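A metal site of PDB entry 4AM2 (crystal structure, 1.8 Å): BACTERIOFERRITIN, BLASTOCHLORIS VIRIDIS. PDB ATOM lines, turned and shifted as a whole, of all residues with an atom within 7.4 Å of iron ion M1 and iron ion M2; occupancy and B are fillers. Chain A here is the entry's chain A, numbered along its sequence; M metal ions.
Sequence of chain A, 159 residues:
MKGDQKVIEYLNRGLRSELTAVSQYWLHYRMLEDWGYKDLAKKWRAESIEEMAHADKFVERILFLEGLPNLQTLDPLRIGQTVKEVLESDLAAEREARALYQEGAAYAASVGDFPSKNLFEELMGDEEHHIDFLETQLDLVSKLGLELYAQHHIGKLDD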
ATOM      1  N   GLY A  14      -0.596 -10.469  13.488  1.00  0.00           N
ATOM      2  CA  GLY A  14      -1.720 -11.257  12.942  1.00  0.00           C
ATOM      3  C   GLY A  14      -1.694 -12.657  13.579  1.00  0.00           C
ATOM      4  O   GLY A  14      -2.733 -13.214  13.943  1.00  0.00           O
ATOM      5  N   SER A  17      -3.144 -12.549  16.885  1.00  0.00           N
ATOM      6  CA  SER A  17      -4.576 -12.344  16.854  1.00  0.00           C
ATOM      7  C   SER A  17      -5.254 -13.719  16.551  1.00  0.00           C
ATOM      8  O   SER A  17      -6.247 -14.076  17.209  1.00  0.00           O
ATOM      9  CB  SER A  17      -4.844 -11.293  15.717  1.00  0.00           C
ATOM     10  OG  SER A  17      -6.234 -11.123  15.653  1.00  0.00           O
ATOM     11  N   GLU A  18      -4.691 -14.513  15.618  1.00  0.00           N
ATOM     12  CA  GLU A  18      -5.261 -15.801  15.258  1.00  0.00           C
ATOM     13  C   GLU A  18      -5.086 -16.752  16.421  1.00  0.00           C
ATOM     14  O   GLU A  18      -5.996 -17.561  16.658  1.00  0.00           O
ATOM     15  CB  GLU A  18      -4.554 -16.347  14.009  1.00  0.00           C
ATOM     16  CG  GLU A  18      -4.921 -15.606  12.693  1.00  0.00           C
ATOM     17  CD  GLU A  18      -6.429 -15.734  12.394  1.00  0.00           C
ATOM     18  OE1 GLU A  18      -7.150 -16.619  12.929  1.00  0.00           O
ATOM     19  OE2 GLU A  18      -6.899 -14.946  11.601  1.00  0.00           O
ATOM     20  N   ALA A  21      -7.774 -16.058  18.724  1.00  0.00           N
ATOM     21  CA  ALA A  21      -9.120 -16.492  18.249  1.00  0.00           C
ATOM     22  C   ALA A  21      -9.219 -18.025  18.340  1.00  0.00           C
ATOM     23  O   ALA A  21     -10.289 -18.589  18.629  1.00  0.00           O
ATOM     24  CB  ALA A  21      -9.347 -16.068  16.802  1.00  0.00           C
ATOM     25  N   TYR A  25     -12.324 -19.279  20.529  1.00  0.00           N
ATOM     26  CA  TYR A  25     -13.349 -20.089  19.894  1.00  0.00           C
ATOM     27  C   TYR A  25     -13.365 -21.490  20.489  1.00  0.00           C
ATOM     28  O   TYR A  25     -14.457 -22.069  20.683  1.00  0.00           O
ATOM     29  CB  TYR A  25     -13.145 -20.215  18.369  1.00  0.00           C
ATOM     30  CG  TYR A  25     -13.674 -19.024  17.555  1.00  0.00           C
ATOM     31  CD1 TYR A  25     -15.028 -18.667  17.650  1.00  0.00           C
ATOM     32  CD2 TYR A  25     -12.855 -18.313  16.694  1.00  0.00           C
ATOM     33  CE1 TYR A  25     -15.567 -17.601  16.898  1.00  0.00           C
ATOM     34  CE2 TYR A  25     -13.354 -17.214  15.917  1.00  0.00           C
ATOM     35  CZ  TYR A  25     -14.690 -16.889  16.025  1.00  0.00           C
ATOM     36  OH  TYR A  25     -15.261 -15.858  15.307  1.00  0.00           O
ATOM     37  N   GLU A  47     -15.281 -23.102  13.573  1.00  0.00           N
ATOM     38  CA  GLU A  47     -14.664 -21.754  13.483  1.00  0.00           C
ATOM     39  C   GLU A  47     -13.253 -21.771  14.084  1.00  0.00           C
ATOM     40  O   GLU A  47     -12.303 -21.194  13.481  1.00  0.00           O
ATOM     41  CB  GLU A  47     -15.435 -20.710  14.254  1.00  0.00           C
ATOM     42  CG  GLU A  47     -16.788 -20.311  13.666  1.00  0.00           C
ATOM     43  CD  GLU A  47     -16.772 -19.845  12.202  1.00  0.00           C
ATOM     44  OE1 GLU A  47     -15.732 -19.915  11.487  1.00  0.00           O
ATOM     45  OE2 GLU A  47     -17.867 -19.394  11.755  1.00  0.00           O
ATOM     46  N   GLU A  50     -10.916 -23.354  11.614  1.00  0.00           N
ATOM     47  CA  GLU A  50     -10.627 -22.344  10.557  1.00  0.00           C
ATOM     48  C   GLU A  50      -9.538 -21.370  10.976  1.00  0.00           C
ATOM     49  O   GLU A  50      -8.703 -21.014  10.154  1.00  0.00           O
ATOM     50  CB  GLU A  50     -11.872 -21.568  10.113  1.00  0.00           C
ATOM     51  CG  GLU A  50     -12.810 -22.520   9.413  1.00  0.00           C
ATOM     52  CD  GLU A  50     -14.034 -21.862   8.805  1.00  0.00           C
ATOM     53  OE1 GLU A  50     -14.123 -20.569   8.724  1.00  0.00           O
ATOM     54  OE2 GLU A  50     -14.898 -22.685   8.416  1.00  0.00           O
ATOM     55  N   GLU A  51      -9.588 -20.887  12.217  1.00  0.00           N
ATOM     56  CA  GLU A  51      -8.599 -19.927  12.733  1.00  0.00           C
ATOM     57  C   GLU A  51      -7.243 -20.641  12.878  1.00  0.00           C
ATOM     58  O   GLU A  51      -6.194 -19.959  12.753  1.00  0.00           O
ATOM     59  CB  GLU A  51      -9.030 -19.312  14.085  1.00  0.00           C
ATOM     60  CG  GLU A  51     -10.376 -18.529  14.017  1.00  0.00           C
ATOM     61  CD  GLU A  51     -10.239 -17.209  13.250  1.00  0.00           C
ATOM     62  OE1 GLU A  51      -9.946 -17.235  12.090  1.00  0.00           O
ATOM     63  OE2 GLU A  51     -10.466 -16.080  13.782  1.00  0.00           O
ATOM     64  N   MET A  52      -7.268 -21.967  13.162  1.00  0.00           N
ATOM     65  CA  MET A  52      -5.999 -22.667  13.252  1.00  0.00           C
ATOM     66  C   MET A  52      -5.252 -22.586  11.916  1.00  0.00           C
ATOM     67  O   MET A  52      -4.038 -22.422  11.909  1.00  0.00           O
ATOM     68  CB  MET A  52      -6.122 -24.135  13.691  1.00  0.00           C
ATOM     69  CG  MET A  52      -6.688 -24.195  15.168  1.00  0.00           C
ATOM     70  SD  MET A  52      -7.157 -25.932  15.483  1.00  0.00           S
ATOM     71  CE  MET A  52      -8.334 -25.645  16.837  1.00  0.00           C
ATOM     72  N   ALA A  53      -5.965 -22.774  10.832  1.00  0.00           N
ATOM     73  CA  ALA A  53      -5.398 -22.724   9.509  1.00  0.00           C
ATOM     74  C   ALA A  53      -4.856 -21.329   9.177  1.00  0.00           C
ATOM     75  O   ALA A  53      -3.821 -21.218   8.536  1.00  0.00           O
ATOM     76  CB  ALA A  53      -6.424 -23.253   8.493  1.00  0.00           C
ATOM     77  N   HIS A  54      -5.555 -20.282   9.623  1.00  0.00           N
ATOM     78  CA  HIS A  54      -5.058 -18.876   9.506  1.00  0.00           C
ATOM     79  C   HIS A  54      -3.759 -18.679  10.253  1.00  0.00           C
ATOM     80  O   HIS A  54      -2.837 -18.054   9.693  1.00  0.00           O
ATOM     81  CB  HIS A  54      -6.099 -17.872  10.051  1.00  0.00           C
ATOM     82  CG  HIS A  54      -7.352 -17.802   9.224  1.00  0.00           C
ATOM     83  ND1 HIS A  54      -8.417 -16.993   9.547  1.00  0.00           N
ATOM     84  CD2 HIS A  54      -7.676 -18.410   8.020  1.00  0.00           C
ATOM     85  CE1 HIS A  54      -9.359 -17.099   8.595  1.00  0.00           C
ATOM     86  NE2 HIS A  54      -8.934 -17.992   7.681  1.00  0.00           N
ATOM     87  N   ALA A  55      -3.655 -19.255  11.464  1.00  0.00           N
ATOM     88  CA  ALA A  55      -2.419 -19.090  12.317  1.00  0.00           C
ATOM     89  C   ALA A  55      -1.278 -19.751  11.531  1.00  0.00           C
ATOM     90  O   ALA A  55      -0.201 -19.176  11.429  1.00  0.00           O
ATOM     91  CB  ALA A  55      -2.594 -19.746  13.675  1.00  0.00           C
ATOM     92  N   PHE A  58       0.166 -17.673   8.742  1.00  0.00           N
ATOM     93  CA  PHE A  58       1.067 -16.639   9.218  1.00  0.00           C
ATOM     94  C   PHE A  58       2.415 -17.218   9.612  1.00  0.00           C
ATOM     95  O   PHE A  58       3.474 -16.632   9.261  1.00  0.00           O
ATOM     96  CB  PHE A  58       0.484 -15.853  10.417  1.00  0.00           C
ATOM     97  CG  PHE A  58      -0.522 -14.823  10.030  1.00  0.00           C
ATOM     98  CD1 PHE A  58      -0.198 -13.823   9.086  1.00  0.00           C
ATOM     99  CD2 PHE A  58      -1.764 -14.813  10.648  1.00  0.00           C
ATOM    100  CE1 PHE A  58      -1.108 -12.834   8.756  1.00  0.00           C
ATOM    101  CE2 PHE A  58      -2.667 -13.809  10.387  1.00  0.00           C
ATOM    102  CZ  PHE A  58      -2.343 -12.803   9.436  1.00  0.00           C
ATOM    103  N   ASP A  90     -16.835 -12.827  20.838  1.00  0.00           N
ATOM    104  CA  ASP A  90     -16.223 -13.219  19.555  1.00  0.00           C
ATOM    105  C   ASP A  90     -16.349 -12.154  18.511  1.00  0.00           C
ATOM    106  O   ASP A  90     -15.436 -11.936  17.724  1.00  0.00           O
ATOM    107  CB  ASP A  90     -16.775 -14.552  19.112  1.00  0.00           C
ATOM    108  CG  ASP A  90     -16.251 -15.701  20.006  1.00  0.00           C
ATOM    109  OD1 ASP A  90     -15.131 -15.585  20.597  1.00  0.00           O
ATOM    110  OD2 ASP A  90     -16.954 -16.732  20.118  1.00  0.00           O
ATOM    111  N   ALA A  93     -13.714  -9.485  19.046  1.00  0.00           N
ATOM    112  CA  ALA A  93     -12.364  -9.930  18.691  1.00  0.00           C
ATOM    113  C   ALA A  93     -12.245  -9.920  17.157  1.00  0.00           C
ATOM    114  O   ALA A  93     -11.193  -9.523  16.590  1.00  0.00           O
ATOM    115  CB  ALA A  93     -11.995 -11.308  19.251  1.00  0.00           C
ATOM    116  N   GLU A  94     -13.308 -10.323  16.463  1.00  0.00           N
ATOM    117  CA  GLU A  94     -13.232 -10.363  15.019  1.00  0.00           C
ATOM    118  C   GLU A  94     -13.127  -8.972  14.427  1.00  0.00           C
ATOM    119  O   GLU A  94     -12.398  -8.793  13.455  1.00  0.00           O
ATOM    120  CB  GLU A  94     -14.473 -11.018  14.352  1.00  0.00           C
ATOM    121  CG  GLU A  94     -14.477 -12.521  14.648  1.00  0.00           C
ATOM    122  CD  GLU A  94     -13.519 -13.269  13.728  1.00  0.00           C
ATOM    123  OE1 GLU A  94     -12.942 -12.595  12.766  1.00  0.00           O
ATOM    124  OE2 GLU A  94     -13.343 -14.510  13.938  1.00  0.00           O
ATOM    125  N   ALA A  97      -9.512  -8.011  14.733  1.00  0.00           N
ATOM    126  CA  ALA A  97      -8.706  -8.789  13.732  1.00  0.00           C
ATOM    127  C   ALA A  97      -8.895  -8.219  12.297  1.00  0.00           C
ATOM    128  O   ALA A  97      -7.926  -8.070  11.541  1.00  0.00           O
ATOM    129  CB  ALA A  97      -9.070 -10.308  13.783  1.00  0.00           C
ATOM    130  N   TYR A 101      -5.923  -6.680   9.910  1.00  0.00           N
ATOM    131  CA  TYR A 101      -5.553  -7.149   8.570  1.00  0.00           C
ATOM    132  C   TYR A 101      -5.692  -6.074   7.522  1.00  0.00           C
ATOM    133  O   TYR A 101      -4.927  -6.054   6.566  1.00  0.00           O
ATOM    134  CB  TYR A 101      -6.391  -8.380   8.170  1.00  0.00           C
ATOM    135  CG  TYR A 101      -6.186  -9.549   9.170  1.00  0.00           C
ATOM    136  CD1 TYR A 101      -5.078  -9.571  10.029  1.00  0.00           C
ATOM    137  CD2 TYR A 101      -7.144 -10.575   9.289  1.00  0.00           C
ATOM    138  CE1 TYR A 101      -4.936 -10.571  10.983  1.00  0.00           C
ATOM    139  CE2 TYR A 101      -7.016 -11.594  10.239  1.00  0.00           C
ATOM    140  CZ  TYR A 101      -5.905 -11.612  11.047  1.00  0.00           C
ATOM    141  OH  TYR A 101      -5.756 -12.621  11.951  1.00  0.00           O
ATOM    142  N   LEU A 123      -7.417 -12.979   4.383  1.00  0.00           N
ATOM    143  CA  LEU A 123      -7.871 -13.154   5.752  1.00  0.00           C
ATOM    144  C   LEU A 123      -8.865 -12.072   6.164  1.00  0.00           C
ATOM    145  O   LEU A 123      -9.778 -12.321   6.950  1.00  0.00           O
ATOM    146  CB  LEU A 123      -6.652 -13.188   6.694  1.00  0.00           C
ATOM    147  CG  LEU A 123      -5.749 -14.399   6.586  1.00  0.00           C
ATOM    148  CD1 LEU A 123      -4.734 -14.322   7.728  1.00  0.00           C
ATOM    149  CD2 LEU A 123      -6.553 -15.601   6.785  1.00  0.00           C
ATOM    150  N   ASP A 126     -12.120 -13.375   5.047  1.00  0.00           N
ATOM    151  CA  ASP A 126     -12.595 -14.444   5.872  1.00  0.00           C
ATOM    152  C   ASP A 126     -13.155 -13.928   7.216  1.00  0.00           C
ATOM    153  O   ASP A 126     -14.170 -14.431   7.698  1.00  0.00           O
ATOM    154  CB  ASP A 126     -11.436 -15.365   6.209  1.00  0.00           C
ATOM    155  CG  ASP A 126     -10.924 -16.152   4.996  1.00  0.00           C
ATOM    156  OD1 ASP A 126     -11.688 -16.230   4.001  1.00  0.00           O
ATOM    157  OD2 ASP A 126      -9.770 -16.750   5.032  1.00  0.00           O
ATOM    158  N   GLU A 127     -12.458 -12.996   7.830  1.00  0.00           N
ATOM    159  CA  GLU A 127     -12.953 -12.431   9.083  1.00  0.00           C
ATOM    160  C   GLU A 127     -14.274 -11.680   8.889  1.00  0.00           C
ATOM    161  O   GLU A 127     -15.149 -11.739   9.783  1.00  0.00           O
ATOM    162  CB  GLU A 127     -11.957 -11.437   9.726  1.00  0.00           C
ATOM    163  CG  GLU A 127     -10.572 -11.991  10.006  1.00  0.00           C
ATOM    164  CD  GLU A 127     -10.556 -13.352  10.707  1.00  0.00           C
ATOM    165  OE1 GLU A 127     -11.452 -13.646  11.519  1.00  0.00           O
ATOM    166  OE2 GLU A 127      -9.621 -14.121  10.449  1.00  0.00           O
ATOM    167  N   GLU A 128     -14.465 -11.082   7.727  1.00  0.00           N
ATOM    168  CA  GLU A 128     -15.770 -10.457   7.471  1.00  0.00           C
ATOM    169  C   GLU A 128     -16.906 -11.500   7.398  1.00  0.00           C
ATOM    170  O   GLU A 128     -17.983 -11.193   7.868  1.00  0.00           O
ATOM    171  CB  GLU A 128     -15.716  -9.526   6.220  1.00  0.00           C
ATOM    172  CG  GLU A 128     -15.056  -8.183   6.657  1.00  0.00           C
ATOM    173  CD  GLU A 128     -15.088  -7.101   5.574  1.00  0.00           C
ATOM    174  OE1 GLU A 128     -15.650  -7.311   4.482  1.00  0.00           O
ATOM    175  OE2 GLU A 128     -14.486  -5.972   5.773  1.00  0.00           O
ATOM    176  N   HIS A 129     -16.645 -12.698   6.897  1.00  0.00           N
ATOM    177  CA  HIS A 129     -17.635 -13.764   6.910  1.00  0.00           C
ATOM    178  C   HIS A 129     -17.945 -14.163   8.371  1.00  0.00           C
ATOM    179  O   HIS A 129     -19.129 -14.337   8.696  1.00  0.00           O
ATOM    180  CB  HIS A 129     -17.189 -14.980   6.132  1.00  0.00           C
ATOM    181  CG  HIS A 129     -17.193 -14.809   4.653  1.00  0.00           C
ATOM    182  ND1 HIS A 129     -18.322 -14.426   3.952  1.00  0.00           N
ATOM    183  CD2 HIS A 129     -16.177 -15.011   3.679  1.00  0.00           C
ATOM    184  CE1 HIS A 129     -18.019 -14.360   2.619  1.00  0.00           C
ATOM    185  NE2 HIS A 129     -16.716 -14.700   2.458  1.00  0.00           N
ATOM    186  N   HIS A 130     -16.921 -14.278   9.212  1.00  0.00           N
ATOM    187  CA  HIS A 130     -17.122 -14.483  10.647  1.00  0.00           C
ATOM    188  C   HIS A 130     -17.969 -13.407  11.271  1.00  0.00           C
ATOM    189  O   HIS A 130     -18.848 -13.724  12.089  1.00  0.00           O
ATOM    190  CB  HIS A 130     -15.808 -14.691  11.454  1.00  0.00           C
ATOM    191  CG  HIS A 130     -14.994 -15.876  10.989  1.00  0.00           C
ATOM    192  ND1 HIS A 130     -13.711 -16.098  11.360  1.00  0.00           N
ATOM    193  CD2 HIS A 130     -15.308 -16.916  10.080  1.00  0.00           C
ATOM    194  CE1 HIS A 130     -13.235 -17.209  10.775  1.00  0.00           C
ATOM    195  NE2 HIS A 130     -14.180 -17.718   9.981  1.00  0.00           N
ATOM    196  N   ILE A 131     -17.673 -12.135  10.977  1.00  0.00           N
ATOM    197  CA  ILE A 131     -18.418 -10.997  11.521  1.00  0.00           C
ATOM    198  C   ILE A 131     -19.907 -11.087  11.080  1.00  0.00           C
ATOM    199  O   ILE A 131     -20.841 -10.904  11.871  1.00  0.00           O
ATOM    200  CB  ILE A 131     -17.764  -9.691  11.050  1.00  0.00           C
ATOM    201  CG1 ILE A 131     -16.482  -9.441  11.874  1.00  0.00           C
ATOM    202  CG2 ILE A 131     -18.708  -8.490  11.272  1.00  0.00           C
ATOM    203  CD1 ILE A 131     -15.677  -8.333  11.218  1.00  0.00           C
ATOM    204  N   LEU A 134     -21.640 -13.784  13.118  1.00  0.00           N
ATOM    205  CA  LEU A 134     -21.870 -13.395  14.520  1.00  0.00           C
ATOM    206  C   LEU A 134     -22.935 -12.315  14.617  1.00  0.00           C
ATOM    207  O   LEU A 134     -23.815 -12.366  15.517  1.00  0.00           O
ATOM    208  CB  LEU A 134     -20.574 -12.895  15.165  1.00  0.00           C
ATOM    209  CG  LEU A 134     -19.545 -14.018  15.315  1.00  0.00           C
ATOM    210  CD1 LEU A 134     -18.169 -13.391  15.587  1.00  0.00           C
ATOM    211  CD2 LEU A 134     -20.000 -15.062  16.382  1.00  0.00           C
HETATM  212 FE    FE M   1      -8.722 -15.861  11.161  1.00  0.00          FE
HETATM  213 FE    FE M   2     -12.434 -15.266  12.451  1.00  0.00          FE
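ND1 of His 130 is bound to iron ion M2 (1.9 Å). Iron ion M2 is bound by OE2 of Glu 94. Iron ion M2 is bound by the side-chain carboxylate (OE1) of Glu 127, 2.1 Å away. The side-chain carboxylate (OE2) of Glu 51 binds iron ion M2. Iron ion M2 has four donor atoms within binding distance. Slightly farther from iron ion M2 lies the side-chain carboxylate (OE1) of Glu 94 (2.7 Å).
Iron ion M1 is bound by a ring nitrogen (ND1) of His 54, the side-chain carboxylate (OE1) of Glu 51, the side-chain carboxylate (OE2) of Glu 127, the side-chain carboxylate (OE2) of Glu 18 and the side-chain carboxylate (OE1) of Glu 18.
A ring nitrogen (NE2) of His 130 sits at hydrogen-bond distance from the side-chain carboxylate of Glu 50 (3.1 Å). A ring nitrogen (NE2) of His 130 sits at hydrogen-bond distance from the side-chain carboxylate (OE1) of Glu 47. The side-chain carboxylate of Glu 94 lies close to the side-chain hydroxyl of Tyr 25 (2.7 Å). A ring nitrogen (NE2) of His 54 lies within hydrogen-bond range of the side-chain carboxylate (OD2) of Asp 126 (3.0 Å). OH of Tyr 101 sits close to OE2 of Glu 18 (2.6 Å).
Within 4 Å of iron ion M2: Glu 51, Glu 94, Glu 127 and His 130.
Within 4 Å of iron ion M1: Glu 18, Glu 51, His 54 and Glu 127. The nearest printed residue that does not touch iron ion M1 is Tyr 101 (4.5 Å).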
